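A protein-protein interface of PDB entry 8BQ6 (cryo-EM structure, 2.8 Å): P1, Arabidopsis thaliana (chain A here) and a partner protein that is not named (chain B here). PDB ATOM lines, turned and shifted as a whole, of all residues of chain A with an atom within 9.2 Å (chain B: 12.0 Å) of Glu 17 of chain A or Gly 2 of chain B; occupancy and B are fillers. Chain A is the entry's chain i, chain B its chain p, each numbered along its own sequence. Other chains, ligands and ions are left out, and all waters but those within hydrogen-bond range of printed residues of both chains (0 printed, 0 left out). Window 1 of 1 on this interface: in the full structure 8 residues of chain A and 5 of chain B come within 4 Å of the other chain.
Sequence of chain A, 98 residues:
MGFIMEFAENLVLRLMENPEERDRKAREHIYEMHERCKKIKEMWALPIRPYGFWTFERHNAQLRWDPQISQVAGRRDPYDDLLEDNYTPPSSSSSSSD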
ATOM      1  N   ASN A  10      19.378  28.487 -14.405  1.00  0.00           N
ATOM      2  CA  ASN A  10      19.090  28.418 -15.836  1.00  0.00           C
ATOM      3  C   ASN A  10      20.349  28.611 -16.666  1.00  0.00           C
ATOM      4  O   ASN A  10      20.561  27.905 -17.660  1.00  0.00           O
ATOM      5  CB  ASN A  10      18.056  29.472 -16.219  1.00  0.00           C
ATOM      6  CG  ASN A  10      16.886  29.504 -15.275  1.00  0.00           C
ATOM      7  OD1 ASN A  10      16.353  28.464 -14.890  1.00  0.00           O
ATOM      8  ND2 ASN A  10      16.479  30.704 -14.884  1.00  0.00           N
ATOM      9  N   LEU A  11      21.191  29.574 -16.282  1.00  0.00           N
ATOM     10  CA  LEU A  11      22.368  29.884 -17.083  1.00  0.00           C
ATOM     11  C   LEU A  11      23.303  28.686 -17.186  1.00  0.00           C
ATOM     12  O   LEU A  11      23.814  28.383 -18.270  1.00  0.00           O
ATOM     13  CB  LEU A  11      23.103  31.086 -16.495  1.00  0.00           C
ATOM     14  CG  LEU A  11      24.365  31.464 -17.274  1.00  0.00           C
ATOM     15  CD1 LEU A  11      24.067  31.574 -18.761  1.00  0.00           C
ATOM     16  CD2 LEU A  11      24.972  32.749 -16.748  1.00  0.00           C
ATOM     17  N   VAL A  12      23.543  27.992 -16.073  1.00  0.00           N
ATOM     18  CA  VAL A  12      24.366  26.788 -16.136  1.00  0.00           C
ATOM     19  C   VAL A  12      23.668  25.705 -16.946  1.00  0.00           C
ATOM     20  O   VAL A  12      24.298  25.016 -17.755  1.00  0.00           O
ATOM     21  CB  VAL A  12      24.726  26.294 -14.723  1.00  0.00           C
ATOM     22  CG1 VAL A  12      25.638  25.093 -14.824  1.00  0.00           C
ATOM     23  CG2 VAL A  12      25.412  27.392 -13.936  1.00  0.00           C
ATOM     24  N   LEU A  13      22.358  25.535 -16.741  1.00  0.00           N
ATOM     25  CA  LEU A  13      21.611  24.520 -17.483  1.00  0.00           C
ATOM     26  C   LEU A  13      21.681  24.769 -18.983  1.00  0.00           C
ATOM     27  O   LEU A  13      21.713  23.822 -19.777  1.00  0.00           O
ATOM     28  CB  LEU A  13      20.156  24.493 -17.021  1.00  0.00           C
ATOM     29  CG  LEU A  13      19.790  23.724 -15.753  1.00  0.00           C
ATOM     30  CD1 LEU A  13      18.297  23.498 -15.720  1.00  0.00           C
ATOM     31  CD2 LEU A  13      20.523  22.400 -15.698  1.00  0.00           C
ATOM     32  N   ARG A  14      21.737  26.042 -19.382  1.00  0.00           N
ATOM     33  CA  ARG A  14      21.852  26.389 -20.823  1.00  0.00           C
ATOM     34  C   ARG A  14      23.247  26.025 -21.337  1.00  0.00           C
ATOM     35  O   ARG A  14      23.366  25.725 -22.542  1.00  0.00           O
ATOM     36  CB  ARG A  14      21.618  27.889 -21.020  1.00  0.00           C
ATOM     37  CG  ARG A  14      20.854  28.240 -22.287  1.00  0.00           C
ATOM     38  CD  ARG A  14      20.001  29.477 -22.090  1.00  0.00           C
ATOM     39  NE  ARG A  14      18.764  29.177 -21.383  1.00  0.00           N
ATOM     40  CZ  ARG A  14      18.444  29.641 -20.179  1.00  0.00           C
ATOM     41  NH1 ARG A  14      19.273  30.439 -19.529  1.00  0.00           N
ATOM     42  NH2 ARG A  14      17.291  29.303 -19.632  1.00  0.00           N
ATOM     43  N   LEU A  15      24.256  26.042 -20.464  1.00  0.00           N
ATOM     44  CA  LEU A  15      25.627  25.801 -20.900  1.00  0.00           C
ATOM     45  C   LEU A  15      25.959  24.320 -21.033  1.00  0.00           C
ATOM     46  O   LEU A  15      26.837  23.969 -21.826  1.00  0.00           O
ATOM     47  CB  LEU A  15      26.600  26.463 -19.927  1.00  0.00           C
ATOM     48  CG  LEU A  15      26.686  27.988 -19.951  1.00  0.00           C
ATOM     49  CD1 LEU A  15      27.472  28.473 -18.752  1.00  0.00           C
ATOM     50  CD2 LEU A  15      27.333  28.462 -21.237  1.00  0.00           C
ATOM     51  N   MET A  16      25.294  23.450 -20.276  1.00  0.00           N
ATOM     52  CA  MET A  16      25.606  22.027 -20.319  1.00  0.00           C
ATOM     53  C   MET A  16      25.157  21.420 -21.642  1.00  0.00           C
ATOM     54  O   MET A  16      24.177  21.862 -22.245  1.00  0.00           O
ATOM     55  CB  MET A  16      24.931  21.297 -19.158  1.00  0.00           C
ATOM     56  CG  MET A  16      24.947  22.056 -17.849  1.00  0.00           C
ATOM     57  SD  MET A  16      24.551  21.032 -16.423  1.00  0.00           S
ATOM     58  CE  MET A  16      25.936  21.392 -15.349  1.00  0.00           C
ATOM     59  N   GLU A  17      25.881  20.400 -22.097  1.00  0.00           N
ATOM     60  CA  GLU A  17      25.497  19.723 -23.325  1.00  0.00           C
ATOM     61  C   GLU A  17      24.303  18.804 -23.066  1.00  0.00           C
ATOM     62  O   GLU A  17      24.043  18.376 -21.939  1.00  0.00           O
ATOM     63  CB  GLU A  17      26.679  18.943 -23.906  1.00  0.00           C
ATOM     64  CG  GLU A  17      27.328  17.956 -22.953  1.00  0.00           C
ATOM     65  CD  GLU A  17      28.653  17.418 -23.473  1.00  0.00           C
ATOM     66  OE1 GLU A  17      28.834  17.351 -24.708  1.00  0.00           O
ATOM     67  OE2 GLU A  17      29.510  17.056 -22.641  1.00  0.00           O
ATOM     68  N   ASN A  18      23.560  18.516 -24.129  1.00  0.00           N
ATOM     69  CA  ASN A  18      22.380  17.663 -24.021  1.00  0.00           C
ATOM     70  C   ASN A  18      22.800  16.219 -23.774  1.00  0.00           C
ATOM     71  O   ASN A  18      23.587  15.673 -24.555  1.00  0.00           O
ATOM     72  CB  ASN A  18      21.545  17.753 -25.290  1.00  0.00           C
ATOM     73  CG  ASN A  18      20.103  17.357 -25.065  1.00  0.00           C
ATOM     74  OD1 ASN A  18      19.551  17.560 -23.985  1.00  0.00           O
ATOM     75  ND2 ASN A  18      19.484  16.785 -26.088  1.00  0.00           N
ATOM     76  N   PRO A  19      22.303  15.567 -22.718  1.00  0.00           N
ATOM     77  CA  PRO A  19      22.766  14.197 -22.435  1.00  0.00           C
ATOM     78  C   PRO A  19      22.384  13.199 -23.510  1.00  0.00           C
ATOM     79  O   PRO A  19      23.188  12.320 -23.849  1.00  0.00           O
ATOM     80  CB  PRO A  19      22.096  13.858 -21.094  1.00  0.00           C
ATOM     81  CG  PRO A  19      21.379  15.091 -20.651  1.00  0.00           C
ATOM     82  CD  PRO A  19      21.230  16.000 -21.811  1.00  0.00           C
ATOM     83  N   GLU A  20      21.174  13.313 -24.060  1.00  0.00           N
ATOM     84  CA  GLU A  20      20.690  12.321 -25.014  1.00  0.00           C
ATOM     85  C   GLU A  20      21.486  12.360 -26.311  1.00  0.00           C
ATOM     86  O   GLU A  20      21.878  11.316 -26.842  1.00  0.00           O
ATOM     87  CB  GLU A  20      19.206  12.546 -25.286  1.00  0.00           C
ATOM     88  CG  GLU A  20      18.462  13.169 -24.125  1.00  0.00           C
ATOM     89  CD  GLU A  20      16.971  12.945 -24.227  1.00  0.00           C
ATOM     90  OE1 GLU A  20      16.213  13.612 -23.494  1.00  0.00           O
ATOM     91  OE2 GLU A  20      16.563  12.098 -25.048  1.00  0.00           O
ATOM     92  N   GLU A  21      21.736  13.560 -26.839  1.00  0.00           N
ATOM     93  CA  GLU A  21      22.519  13.686 -28.066  1.00  0.00           C
ATOM     94  C   GLU A  21      23.972  13.296 -27.839  1.00  0.00           C
ATOM     95  O   GLU A  21      24.610  12.694 -28.715  1.00  0.00           O
ATOM     96  CB  GLU A  21      22.431  15.115 -28.593  1.00  0.00           C
ATOM     97  CG  GLU A  21      22.200  15.204 -30.084  1.00  0.00           C
ATOM     98  CD  GLU A  21      20.930  14.503 -30.512  1.00  0.00           C
ATOM     99  OE1 GLU A  21      19.836  15.018 -30.206  1.00  0.00           O
ATOM    100  OE2 GLU A  21      21.024  13.443 -31.158  1.00  0.00           O
ATOM    101  N   ARG A  22      24.514  13.648 -26.674  1.00  0.00           N
ATOM    102  CA  ARG A  22      25.891  13.297 -26.354  1.00  0.00           C
ATOM    103  C   ARG A  22      26.067  11.784 -26.289  1.00  0.00           C
ATOM    104  O   ARG A  22      27.069  11.244 -26.770  1.00  0.00           O
ATOM    105  CB  ARG A  22      26.296  13.958 -25.037  1.00  0.00           C
ATOM    106  CG  ARG A  22      27.747  13.768 -24.668  1.00  0.00           C
ATOM    107  CD  ARG A  22      27.890  13.017 -23.359  1.00  0.00           C
ATOM    108  NE  ARG A  22      27.457  13.812 -22.216  1.00  0.00           N
ATOM    109  CZ  ARG A  22      26.505  13.449 -21.368  1.00  0.00           C
ATOM    110  NH1 ARG A  22      25.868  12.296 -21.496  1.00  0.00           N
ATOM    111  NH2 ARG A  22      26.189  14.258 -20.362  1.00  0.00           N
ATOM    112  N   ASP A  23      25.102  11.080 -25.691  1.00  0.00           N
ATOM    113  CA  ASP A  23      25.173   9.621 -25.674  1.00  0.00           C
ATOM    114  C   ASP A  23      24.913   9.028 -27.053  1.00  0.00           C
ATOM    115  O   ASP A  23      25.537   8.025 -27.426  1.00  0.00           O
ATOM    116  CB  ASP A  23      24.181   9.049 -24.663  1.00  0.00           C
ATOM    117  CG  ASP A  23      24.393   9.587 -23.258  1.00  0.00           C
ATOM    118  OD1 ASP A  23      25.557   9.766 -22.841  1.00  0.00           O
ATOM    119  OD2 ASP A  23      23.385   9.829 -22.566  1.00  0.00           O
ATOM    120  N   LYS A  25      25.625  10.303 -30.080  1.00  0.00           N
ATOM    121  CA  LYS A  25      26.843  10.441 -30.920  1.00  0.00           C
ATOM    122  C   LYS A  25      27.933   9.476 -30.437  1.00  0.00           C
ATOM    123  O   LYS A  25      28.651   8.948 -31.294  1.00  0.00           O
ATOM    124  CB  LYS A  25      27.304  11.900 -30.915  1.00  0.00           C
ATOM    125  CG  LYS A  25      26.491  12.848 -31.782  1.00  0.00           C
ATOM    126  CD  LYS A  25      26.919  14.292 -31.645  1.00  0.00           C
ATOM    127  CE  LYS A  25      26.924  14.779 -30.212  1.00  0.00           C
ATOM    128  NZ  LYS A  25      27.757  15.994 -30.046  1.00  0.00           N
ATOM    129  N   GLY B   2      22.159  22.689 -24.224  1.00  0.00           N
ATOM    130  CA  GLY B   2      21.194  22.829 -23.148  1.00  0.00           C
ATOM    131  C   GLY B   2      20.785  21.512 -22.523  1.00  0.00           C
ATOM    132  O   GLY B   2      20.817  20.468 -23.172  1.00  0.00           O
ATOM    133  N   ARG B   3      20.396  21.570 -21.253  1.00  0.00           N
ATOM    134  CA  ARG B   3      19.957  20.409 -20.492  1.00  0.00           C
ATOM    135  C   ARG B   3      18.713  20.777 -19.695  1.00  0.00           C
ATOM    136  O   ARG B   3      18.628  21.872 -19.130  1.00  0.00           O
ATOM    137  CB  ARG B   3      21.081  19.919 -19.563  1.00  0.00           C
ATOM    138  CG  ARG B   3      20.619  19.329 -18.245  1.00  0.00           C
ATOM    139  CD  ARG B   3      21.798  18.946 -17.365  1.00  0.00           C
ATOM    140  NE  ARG B   3      22.490  17.746 -17.815  1.00  0.00           N
ATOM    141  CZ  ARG B   3      22.134  16.513 -17.484  1.00  0.00           C
ATOM    142  NH1 ARG B   3      21.062  16.279 -16.745  1.00  0.00           N
ATOM    143  NH2 ARG B   3      22.876  15.490 -17.896  1.00  0.00           N
ATOM    144  N   LYS B   4      17.740  19.870 -19.671  1.00  0.00           N
ATOM    145  CA  LYS B   4      16.528  20.094 -18.896  1.00  0.00           C
ATOM    146  C   LYS B   4      16.793  19.898 -17.411  1.00  0.00           C
ATOM    147  O   LYS B   4      17.609  19.067 -17.005  1.00  0.00           O
ATOM    148  CB  LYS B   4      15.417  19.149 -19.347  1.00  0.00           C
ATOM    149  CG  LYS B   4      14.112  19.382 -18.629  1.00  0.00           C
ATOM    150  CD  LYS B   4      12.971  18.628 -19.270  1.00  0.00           C
ATOM    151  CE  LYS B   4      13.126  17.142 -19.008  1.00  0.00           C
ATOM    152  NZ  LYS B   4      11.946  16.353 -19.443  1.00  0.00           N
ATOM    153  N   LYS B   5      16.080  20.671 -16.599  1.00  0.00           N
ATOM    154  CA  LYS B   5      16.218  20.573 -15.155  1.00  0.00           C
ATOM    155  C   LYS B   5      15.718  19.221 -14.664  1.00  0.00           C
ATOM    156  O   LYS B   5      14.877  18.582 -15.302  1.00  0.00           O
ATOM    157  CB  LYS B   5      15.448  21.709 -14.479  1.00  0.00           C
ATOM    158  CG  LYS B   5      15.679  21.832 -12.977  1.00  0.00           C
ATOM    159  CD  LYS B   5      15.246  23.189 -12.438  1.00  0.00           C
ATOM    160  CE  LYS B   5      14.099  23.781 -13.238  1.00  0.00           C
ATOM    161  NZ  LYS B   5      12.780  23.404 -12.659  1.00  0.00           N
ATOM    162  N   GLY B   6      16.256  18.776 -13.537  1.00  0.00           N
ATOM    163  CA  GLY B   6      15.815  17.555 -12.896  1.00  0.00           C
ATOM    164  C   GLY B   6      16.942  16.555 -12.749  1.00  0.00           C
ATOM    165  O   GLY B   6      18.059  16.746 -13.226  1.00  0.00           O
ATOM    166  N   LEU B   7      16.617  15.470 -12.059  1.00  0.00           N
ATOM    167  CA  LEU B   7      17.586  14.417 -11.837  1.00  0.00           C
ATOM    168  C   LEU B   7      17.873  13.683 -13.146  1.00  0.00           C
ATOM    169  O   LEU B   7      17.016  13.620 -14.032  1.00  0.00           O
ATOM    170  CB  LEU B   7      17.066  13.444 -10.785  1.00  0.00           C
ATOM    171  CG  LEU B   7      18.047  13.007  -9.697  1.00  0.00           C
ATOM    172  CD1 LEU B   7      18.440  14.178  -8.815  1.00  0.00           C
ATOM    173  CD2 LEU B   7      17.437  11.894  -8.870  1.00  0.00           C
ATOM    174  N   PRO B   8      19.078  13.139 -13.304  1.00  0.00           N
ATOM    175  CA  PRO B   8      19.377  12.369 -14.517  1.00  0.00           C
ATOM    176  C   PRO B   8      18.458  11.164 -14.642  1.00  0.00           C
ATOM    177  O   PRO B   8      18.023  10.577 -13.649  1.00  0.00           O
ATOM    178  CB  PRO B   8      20.840  11.945 -14.337  1.00  0.00           C
ATOM    179  CG  PRO B   8      21.257  12.379 -12.994  1.00  0.00           C
ATOM    180  CD  PRO B   8      20.237  13.284 -12.409  1.00  0.00           C
ATOM    181  N   GLU B   9      18.145  10.810 -15.884  1.00  0.00           N
ATOM    182  CA  GLU B   9      17.258   9.697 -16.191  1.00  0.00           C
ATOM    183  C   GLU B   9      18.029   8.614 -16.930  1.00  0.00           C
ATOM    184  O   GLU B   9      18.772   8.909 -17.872  1.00  0.00           O
ATOM    185  CB  GLU B   9      16.067  10.159 -17.031  1.00  0.00           C
ATOM    186  CG  GLU B   9      14.796  10.349 -16.237  1.00  0.00           C
ATOM    187  CD  GLU B   9      14.448   9.128 -15.413  1.00  0.00           C
ATOM    188  OE1 GLU B   9      14.227   9.278 -14.192  1.00  0.00           O
ATOM    189  OE2 GLU B   9      14.396   8.019 -15.987  1.00  0.00           O
ATOM    190  N   PHE B  10      17.839   7.366 -16.511  1.00  0.00           N
ATOM    191  CA  PHE B  10      18.508   6.224 -17.115  1.00  0.00           C
ATOM    192  C   PHE B  10      17.514   5.085 -17.299  1.00  0.00           C
ATOM    193  O   PHE B  10      16.482   5.017 -16.627  1.00  0.00           O
ATOM    194  CB  PHE B  10      19.700   5.749 -16.269  1.00  0.00           C
ATOM    195  CG  PHE B  10      20.771   6.791 -16.068  1.00  0.00           C
ATOM    196  CD1 PHE B  10      21.671   7.089 -17.080  1.00  0.00           C
ATOM    197  CD2 PHE B  10      20.901   7.444 -14.855  1.00  0.00           C
ATOM    198  CE1 PHE B  10      22.662   8.035 -16.890  1.00  0.00           C
ATOM    199  CE2 PHE B  10      21.889   8.387 -14.660  1.00  0.00           C
ATOM    200  CZ  PHE B  10      22.771   8.683 -15.678  1.00  0.00           C
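NH1 of Arg 14 of chain A is in hydrogen-bond range of O of Asn 10 of chain A (3.4 Å). OE2 of Glu 17 of chain A is in salt-bridge range of NE of Arg 22 of chain A, 3.9 Å away.
Printed residues of chain B that touch a printed residue of chain A: Gly 2, Arg 3 and Lys 5. Printed residues of chain A that touch a printed residue of chain B: Leu 13, Arg 14, Met 16, Glu 17, Asn 18 and Pro 19. Hydrophobic or aromatic side chains of chain A within 4 Å of the printed part of chain B: Leu 13, Met 16 and Pro 19. Among the printed residues, no Asp or Glu carboxylate lies within 4 Å of a Lys or Arg side-chain nitrogen of the other chain.
Among the printed residues, pairs that only touch across the chains: Pro 19 of chain A with Arg 3 of chain B (3.2 Å), Leu 13 of chain A with Gly 2 of chain B (3.6 Å), Met 16 of chain A with Arg 3 of chain B (3.6 Å), Leu 13 of chain A with Lys 5 of chain B (3.6 Å), Arg 14 of chain A with Gly 2 of chain B (3.7 Å) and Glu 17 of chain A with Gly 2 of chain B (3.9 Å).
The backbone carbonyl oxygen (O) of Leu 13 of chain A lies within hydrogen-bond range of the backbone NH (N) of Arg 3 of chain B, at 3.0 Å. The backbone carbonyl oxygen of Met 16 of chain A is in hydrogen-bond range of the backbone NH of Gly 2 of chain B, at 2.9 Å. The side-chain amide oxygen (OD1) of Asn 18 of chain A sits close to the backbone carbonyl oxygen (O) of Gly 2 of chain B (3.3 Å).
Of chain B, only Gly 2 (3.9 Å) comes within 4 Å of Glu 17 of chain A. Printed residues of chain A within 4 Å of Gly 2 of chain B: Leu 13, Arg 14, Met 16, Glu 17 and Asn 18. Of chain B, only Gly 2 (3.6 Å), Arg 3 (3.0 Å) and Lys 5 (3.6 Å) come within 4 Å of Leu 13 of chain A. Of the printed residues of chain A, Lys 5 of chain B touches Leu 13. Of the printed residues of chain A, Arg 3 of chain B touches Leu 13 (3.0 Å), Met 16 (3.6 Å) and Pro 19 (3.2 Å). Leu 15 of chain A touches none of the printed residues of chain B. Pro 8 of chain B touches none of the printed residues of chain A. The nearest residue of chain A that does not touch Gly 2 of chain B is Pro 19 of chain A (4.7 Å). The nearest printed residue of chain A that does not touch Lys 5 of chain B is Asn 10 of chain A (5.5 Å).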
